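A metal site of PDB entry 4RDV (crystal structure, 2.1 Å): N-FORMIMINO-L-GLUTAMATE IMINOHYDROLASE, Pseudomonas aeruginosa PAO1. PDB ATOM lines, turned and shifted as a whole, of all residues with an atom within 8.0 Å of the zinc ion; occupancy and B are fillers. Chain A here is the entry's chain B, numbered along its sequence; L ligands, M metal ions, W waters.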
ATOM      1  N   HIS A  56     -11.809 -14.943   0.571  1.00  0.00           N
ATOM      2  CA  HIS A  56     -11.212 -14.619   1.855  1.00  0.00           C
ATOM      3  C   HIS A  56      -9.788 -15.142   1.982  1.00  0.00           C
ATOM      4  O   HIS A  56      -9.578 -16.353   2.025  1.00  0.00           O
ATOM      5  CB  HIS A  56     -12.055 -15.163   3.009  1.00  0.00           C
ATOM      6  CG  HIS A  56     -11.567 -14.742   4.356  1.00  0.00           C
ATOM      7  ND1 HIS A  56     -11.687 -13.450   4.822  1.00  0.00           N
ATOM      8  CD2 HIS A  56     -10.925 -15.429   5.328  1.00  0.00           C
ATOM      9  CE1 HIS A  56     -11.163 -13.367   6.032  1.00  0.00           C
ATOM     10  NE2 HIS A  56     -10.685 -14.556   6.358  1.00  0.00           N
ATOM     11  N   SER A  57      -8.821 -14.229   2.049  1.00  0.00           N
ATOM     12  CA  SER A  57      -7.391 -14.562   2.165  1.00  0.00           C
ATOM     13  C   SER A  57      -6.619 -13.659   3.126  1.00  0.00           C
ATOM     14  O   SER A  57      -6.825 -12.448   3.142  1.00  0.00           O
ATOM     15  CB  SER A  57      -6.738 -14.453   0.782  1.00  0.00           C
ATOM     16  OG  SER A  57      -5.322 -14.349   0.897  1.00  0.00           O
ATOM     17  N   HIS A  58      -5.718 -14.248   3.926  1.00  0.00           N
ATOM     18  CA  HIS A  58      -4.674 -13.469   4.619  1.00  0.00           C
ATOM     19  C   HIS A  58      -3.316 -13.957   4.128  1.00  0.00           C
ATOM     20  O   HIS A  58      -2.777 -14.915   4.680  1.00  0.00           O
ATOM     21  CB  HIS A  58      -4.718 -13.646   6.146  1.00  0.00           C
ATOM     22  CG  HIS A  58      -6.087 -13.505   6.720  1.00  0.00           C
ATOM     23  ND1 HIS A  58      -6.813 -12.334   6.647  1.00  0.00           N
ATOM     24  CD2 HIS A  58      -6.874 -14.396   7.367  1.00  0.00           C
ATOM     25  CE1 HIS A  58      -7.984 -12.507   7.224  1.00  0.00           C
ATOM     26  NE2 HIS A  58      -8.049 -13.744   7.682  1.00  0.00           N
ATOM     27  N   GLN A  61      -0.115 -15.624   5.954  1.00  0.00           N
ATOM     28  CA  GLN A  61      -0.291 -16.874   6.706  1.00  0.00           C
ATOM     29  C   GLN A  61       0.176 -18.116   5.924  1.00  0.00           C
ATOM     30  O   GLN A  61       0.508 -19.137   6.531  1.00  0.00           O
ATOM     31  CB  GLN A  61      -1.734 -17.010   7.230  1.00  0.00           C
ATOM     32  CG  GLN A  61      -2.105 -15.895   8.227  1.00  0.00           C
ATOM     33  CD  GLN A  61      -3.489 -16.056   8.865  1.00  0.00           C
ATOM     34  OE1 GLN A  61      -4.212 -17.020   8.595  1.00  0.00           O
ATOM     35  NE2 GLN A  61      -3.872 -15.092   9.707  1.00  0.00           N
ATOM     36  N   PHE A  78      -7.735 -22.503  19.142  1.00  0.00           N
ATOM     37  CA  PHE A  78      -7.721 -21.405  18.194  1.00  0.00           C
ATOM     38  C   PHE A  78      -6.881 -20.217  18.700  1.00  0.00           C
ATOM     39  O   PHE A  78      -6.157 -19.571  17.921  1.00  0.00           O
ATOM     40  CB  PHE A  78      -9.182 -20.982  17.969  1.00  0.00           C
ATOM     41  CG  PHE A  78      -9.352 -19.793  17.066  1.00  0.00           C
ATOM     42  CD1 PHE A  78      -9.655 -19.974  15.725  1.00  0.00           C
ATOM     43  CD2 PHE A  78      -9.232 -18.493  17.560  1.00  0.00           C
ATOM     44  CE1 PHE A  78      -9.816 -18.882  14.880  1.00  0.00           C
ATOM     45  CE2 PHE A  78      -9.385 -17.394  16.725  1.00  0.00           C
ATOM     46  CZ  PHE A  78      -9.678 -17.589  15.385  1.00  0.00           C
ATOM     47  N   TRP A  81      -3.112 -20.934  18.666  1.00  0.00           N
ATOM     48  CA  TRP A  81      -2.706 -20.750  17.276  1.00  0.00           C
ATOM     49  C   TRP A  81      -2.571 -19.257  16.938  1.00  0.00           C
ATOM     50  O   TRP A  81      -1.578 -18.837  16.333  1.00  0.00           O
ATOM     51  CB  TRP A  81      -3.690 -21.420  16.315  1.00  0.00           C
ATOM     52  CG  TRP A  81      -3.499 -21.018  14.887  1.00  0.00           C
ATOM     53  CD1 TRP A  81      -2.690 -21.620  13.958  1.00  0.00           C
ATOM     54  CD2 TRP A  81      -4.134 -19.926  14.208  1.00  0.00           C
ATOM     55  NE1 TRP A  81      -2.790 -20.975  12.753  1.00  0.00           N
ATOM     56  CE2 TRP A  81      -3.660 -19.931  12.883  1.00  0.00           C
ATOM     57  CE3 TRP A  81      -5.064 -18.947  14.595  1.00  0.00           C
ATOM     58  CZ2 TRP A  81      -4.073 -18.991  11.944  1.00  0.00           C
ATOM     59  CZ3 TRP A  81      -5.470 -18.022  13.671  1.00  0.00           C
ATOM     60  CH2 TRP A  81      -4.980 -18.044  12.355  1.00  0.00           C
ATOM     61  N   PHE A 119      -8.050  -9.974   2.660  1.00  0.00           N
ATOM     62  CA  PHE A 119      -8.567  -9.415   3.908  1.00  0.00           C
ATOM     63  C   PHE A 119      -7.330  -8.961   4.690  1.00  0.00           C
ATOM     64  O   PHE A 119      -6.738  -9.709   5.477  1.00  0.00           O
ATOM     65  CB  PHE A 119      -9.348 -10.528   4.610  1.00  0.00           C
ATOM     66  CG  PHE A 119     -10.225 -10.080   5.771  1.00  0.00           C
ATOM     67  CD1 PHE A 119      -9.664  -9.780   7.008  1.00  0.00           C
ATOM     68  CD2 PHE A 119     -11.612 -10.098   5.656  1.00  0.00           C
ATOM     69  CE1 PHE A 119     -10.483  -9.423   8.102  1.00  0.00           C
ATOM     70  CE2 PHE A 119     -12.423  -9.772   6.734  1.00  0.00           C
ATOM     71  CZ  PHE A 119     -11.856  -9.432   7.969  1.00  0.00           C
ATOM     72  N   TYR A 121      -4.932  -6.867   7.035  1.00  0.00           N
ATOM     73  CA  TYR A 121      -4.868  -6.101   8.270  1.00  0.00           C
ATOM     74  C   TYR A 121      -3.458  -5.802   8.772  1.00  0.00           C
ATOM     75  O   TYR A 121      -3.300  -5.239   9.844  1.00  0.00           O
ATOM     76  CB  TYR A 121      -5.672  -6.777   9.392  1.00  0.00           C
ATOM     77  CG  TYR A 121      -5.316  -8.236   9.651  1.00  0.00           C
ATOM     78  CD1 TYR A 121      -4.154  -8.589  10.337  1.00  0.00           C
ATOM     79  CD2 TYR A 121      -6.159  -9.254   9.217  1.00  0.00           C
ATOM     80  CE1 TYR A 121      -3.842  -9.916  10.583  1.00  0.00           C
ATOM     81  CE2 TYR A 121      -5.853 -10.600   9.461  1.00  0.00           C
ATOM     82  CZ  TYR A 121      -4.693 -10.920  10.134  1.00  0.00           C
ATOM     83  OH  TYR A 121      -4.394 -12.242  10.378  1.00  0.00           O
ATOM     84  N   HIS A 206     -12.493  -6.018  11.011  1.00  0.00           N
ATOM     85  CA  HIS A 206     -11.875  -7.291  11.334  1.00  0.00           C
ATOM     86  C   HIS A 206     -12.879  -8.268  11.937  1.00  0.00           C
ATOM     87  O   HIS A 206     -12.961  -9.425  11.531  1.00  0.00           O
ATOM     88  CB  HIS A 206     -10.711  -7.150  12.297  1.00  0.00           C
ATOM     89  CG  HIS A 206     -10.070  -8.471  12.614  1.00  0.00           C
ATOM     90  ND1 HIS A 206     -10.416  -9.211  13.728  1.00  0.00           N
ATOM     91  CD2 HIS A 206      -9.146  -9.203  11.948  1.00  0.00           C
ATOM     92  CE1 HIS A 206      -9.713 -10.332  13.734  1.00  0.00           C
ATOM     93  NE2 HIS A 206      -8.930 -10.345  12.670  1.00  0.00           N
ATOM     94  N   ILE A 231     -16.486  -8.939   7.060  1.00  0.00           N
ATOM     95  CA  ILE A 231     -16.220  -9.015   8.493  1.00  0.00           C
ATOM     96  C   ILE A 231     -16.104 -10.493   8.928  1.00  0.00           C
ATOM     97  O   ILE A 231     -16.863 -11.339   8.442  1.00  0.00           O
ATOM     98  CB  ILE A 231     -17.351  -8.287   9.306  1.00  0.00           C
ATOM     99  CG1 ILE A 231     -17.027  -8.200  10.797  1.00  0.00           C
ATOM    100  CG2 ILE A 231     -18.717  -8.957   9.065  1.00  0.00           C
ATOM    101  CD1 ILE A 231     -18.027  -7.318  11.596  1.00  0.00           C
ATOM    102  N   HIS A 232     -15.149 -10.804   9.802  1.00  0.00           N
ATOM    103  CA  HIS A 232     -15.097 -12.126  10.440  1.00  0.00           C
ATOM    104  C   HIS A 232     -16.230 -12.138  11.464  1.00  0.00           C
ATOM    105  O   HIS A 232     -16.321 -11.227  12.282  1.00  0.00           O
ATOM    106  CB  HIS A 232     -13.806 -12.328  11.257  1.00  0.00           C
ATOM    107  CG  HIS A 232     -12.561 -12.553  10.449  1.00  0.00           C
ATOM    108  ND1 HIS A 232     -11.438 -11.775  10.607  1.00  0.00           N
ATOM    109  CD2 HIS A 232     -12.228 -13.513   9.552  1.00  0.00           C
ATOM    110  CE1 HIS A 232     -10.475 -12.223   9.808  1.00  0.00           C
ATOM    111  NE2 HIS A 232     -10.934 -13.269   9.156  1.00  0.00           N
ATOM    112  N   GLU A 235     -16.995 -17.101  14.349  1.00  0.00           N
ATOM    113  CA  GLU A 235     -16.129 -18.225  14.000  1.00  0.00           C
ATOM    114  C   GLU A 235     -15.980 -19.235  15.148  1.00  0.00           C
ATOM    115  O   GLU A 235     -16.023 -20.455  14.927  1.00  0.00           O
ATOM    116  CB  GLU A 235     -14.750 -17.726  13.565  1.00  0.00           C
ATOM    117  CG  GLU A 235     -13.876 -18.818  13.002  1.00  0.00           C
ATOM    118  CD  GLU A 235     -12.500 -18.342  12.587  1.00  0.00           C
ATOM    119  OE1 GLU A 235     -12.197 -17.141  12.765  1.00  0.00           O
ATOM    120  OE2 GLU A 235     -11.714 -19.150  12.065  1.00  0.00           O
ATOM    121  N   VAL A 268     -17.789 -13.630   7.000  1.00  0.00           N
ATOM    122  CA  VAL A 268     -16.790 -14.680   6.864  1.00  0.00           C
ATOM    123  C   VAL A 268     -16.905 -15.646   8.041  1.00  0.00           C
ATOM    124  O   VAL A 268     -16.972 -15.208   9.194  1.00  0.00           O
ATOM    125  CB  VAL A 268     -15.358 -14.087   6.807  1.00  0.00           C
ATOM    126  CG1 VAL A 268     -14.323 -15.197   6.579  1.00  0.00           C
ATOM    127  CG2 VAL A 268     -15.274 -13.050   5.709  1.00  0.00           C
ATOM    128  N   HIS A 269     -16.919 -16.941   7.704  1.00  0.00           N
ATOM    129  CA  HIS A 269     -17.151 -18.053   8.622  1.00  0.00           C
ATOM    130  C   HIS A 269     -18.622 -18.182   9.031  1.00  0.00           C
ATOM    131  O   HIS A 269     -19.293 -19.129   8.615  1.00  0.00           O
ATOM    132  CB  HIS A 269     -16.258 -18.024   9.869  1.00  0.00           C
ATOM    133  CG  HIS A 269     -14.801 -17.874   9.560  1.00  0.00           C
ATOM    134  ND1 HIS A 269     -14.097 -18.792   8.819  1.00  0.00           N
ATOM    135  CD2 HIS A 269     -13.915 -16.897   9.906  1.00  0.00           C
ATOM    136  CE1 HIS A 269     -12.834 -18.395   8.713  1.00  0.00           C
ATOM    137  NE2 HIS A 269     -12.699 -17.250   9.364  1.00  0.00           N
ATOM    138  N   CYS A 291     -14.735 -21.039   4.708  1.00  0.00           N
ATOM    139  CA  CYS A 291     -13.327 -21.362   4.536  1.00  0.00           C
ATOM    140  C   CYS A 291     -13.113 -22.721   5.172  1.00  0.00           C
ATOM    141  O   CYS A 291     -12.658 -22.819   6.312  1.00  0.00           O
ATOM    142  CB  CYS A 291     -12.466 -20.307   5.239  1.00  0.00           C
ATOM    143  SG  CYS A 291     -12.855 -18.607   4.717  1.00  0.00           S
ATOM    144  N   THR A 294      -9.629 -24.248   6.508  1.00  0.00           N
ATOM    145  CA  THR A 294      -9.093 -23.500   7.633  1.00  0.00           C
ATOM    146  C   THR A 294      -9.976 -23.706   8.866  1.00  0.00           C
ATOM    147  O   THR A 294      -9.484 -23.916   9.983  1.00  0.00           O
ATOM    148  CB  THR A 294      -8.929 -21.985   7.296  1.00  0.00           C
ATOM    149  OG1 THR A 294      -7.809 -21.833   6.413  1.00  0.00           O
ATOM    150  CG2 THR A 294      -8.680 -21.173   8.557  1.00  0.00           C
ATOM    151  N   LEU A 298      -8.611 -25.229  12.258  1.00  0.00           N
ATOM    152  CA  LEU A 298      -8.676 -24.470  13.520  1.00  0.00           C
ATOM    153  C   LEU A 298      -9.705 -25.015  14.506  1.00  0.00           C
ATOM    154  O   LEU A 298      -9.851 -24.481  15.606  1.00  0.00           O
ATOM    155  CB  LEU A 298      -8.959 -22.987  13.236  1.00  0.00           C
ATOM    156  CG  LEU A 298      -7.899 -22.255  12.405  1.00  0.00           C
ATOM    157  CD1 LEU A 298      -8.315 -20.795  12.182  1.00  0.00           C
ATOM    158  CD2 LEU A 298      -6.502 -22.357  13.058  1.00  0.00           C
ATOM    159  N   SER A 319      -9.725 -19.482   1.056  1.00  0.00           N
ATOM    160  CA  SER A 319      -8.661 -20.324   1.609  1.00  0.00           C
ATOM    161  C   SER A 319      -8.098 -19.785   2.927  1.00  0.00           C
ATOM    162  O   SER A 319      -7.368 -20.487   3.633  1.00  0.00           O
ATOM    163  CB  SER A 319      -7.553 -20.554   0.566  1.00  0.00           C
ATOM    164  OG  SER A 319      -7.002 -19.321   0.141  1.00  0.00           O
ATOM    165  N   ASP A 320      -8.444 -18.541   3.270  1.00  0.00           N
ATOM    166  CA  ASP A 320      -8.197 -18.005   4.607  1.00  0.00           C
ATOM    167  C   ASP A 320      -6.740 -18.069   5.103  1.00  0.00           C
ATOM    168  O   ASP A 320      -5.914 -17.233   4.730  1.00  0.00           O
ATOM    169  CB  ASP A 320      -9.155 -18.660   5.622  1.00  0.00           C
ATOM    170  CG  ASP A 320      -9.233 -17.907   6.939  1.00  0.00           C
ATOM    171  OD1 ASP A 320      -8.599 -16.848   7.051  1.00  0.00           O
ATOM    172  OD2 ASP A 320      -9.939 -18.369   7.855  1.00  0.00           O
ATOM    173  N   SER A 321      -6.423 -19.068   5.934  1.00  0.00           N
ATOM    174  CA  SER A 321      -5.056 -19.254   6.442  1.00  0.00           C
ATOM    175  C   SER A 321      -4.155 -19.954   5.424  1.00  0.00           C
ATOM    176  O   SER A 321      -2.948 -20.085   5.622  1.00  0.00           O
ATOM    177  CB  SER A 321      -5.067 -20.061   7.745  1.00  0.00           C
ATOM    178  OG  SER A 321      -5.308 -21.438   7.493  1.00  0.00           O
HETATM  179  C1  LIG L   1      -7.299 -13.474  11.658  1.00  0.00           C
HETATM  180  N1  LIG L   1      -8.116 -15.720  11.653  1.00  0.00           N
HETATM  181  O1  LIG L   1      -6.357 -13.934  10.977  1.00  0.00           O
HETATM  182  O2  LIG L   1      -7.392 -12.241  11.855  1.00  0.00           O
HETATM  183  C2  LIG L   1      -8.315 -14.411  12.233  1.00  0.00           C
HETATM  184  C3  LIG L   1      -8.188 -14.413  13.728  1.00  0.00           C
HETATM  185  C4  LIG L   1      -9.069 -16.663  12.140  1.00  0.00           C
HETATM  186  N2  LIG L   1      -9.294 -17.710  11.382  1.00  0.00           N
HETATM  187  C5  LIG L   1      -9.135 -13.544  14.502  1.00  0.00           C
HETATM  188  O3  LIG L   1     -10.343 -13.485  14.159  1.00  0.00           O
HETATM  189  O4  LIG L   1      -8.715 -12.853  15.471  1.00  0.00           O
HETATM  190 ZN    ZN M   1      -9.707 -14.813   8.175  1.00  0.00          ZN
HETATM  191  O   HOH W   1     -10.168 -16.354   9.366  1.00  0.00           O
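N2 of the ligand is in salt-bridge range of OE2 of Glu 235, 2.9 Å away. NE2 of Gln 61 sits at hydrogen-bond distance from O1 of the ligand, at 3.0 Å. A ring nitrogen (NE2) of His 206 is in hydrogen-bond range of an oxygen (O2) of the ligand, 2.6 Å away. A nitrogen (N2) of the ligand lies within salt-bridge range of the side-chain carboxylate (OD2) of Asp 320 (3.6 Å). The side-chain hydroxyl of Tyr 121 is in hydrogen-bond range of an oxygen (O1) of the ligand, at 2.7 Å.
ND1 of His 232 is in hydrogen-bond range of O of His 206, 2.9 Å away. The backbone carbonyl oxygen of Phe 119 lies within hydrogen-bond range of a ring nitrogen (ND1) of His 58 (2.9 Å). O of His 56 lies within hydrogen-bond range of N of Ser 319, 3.3 Å away. OD2 of Asp 320 lies close to NE2 of His 269, at 3.3 Å.
The zinc ion is bound by water W1, NE2 of His 58, NE2 of His 56, NE2 of His 232 and OD1 of Asp 320.
Water W1 lies within hydrogen-bond range of the side-chain carboxylate (OD2) of Asp 320, a nitrogen (N2) of the ligand and a ring nitrogen (NE2) of His 269.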
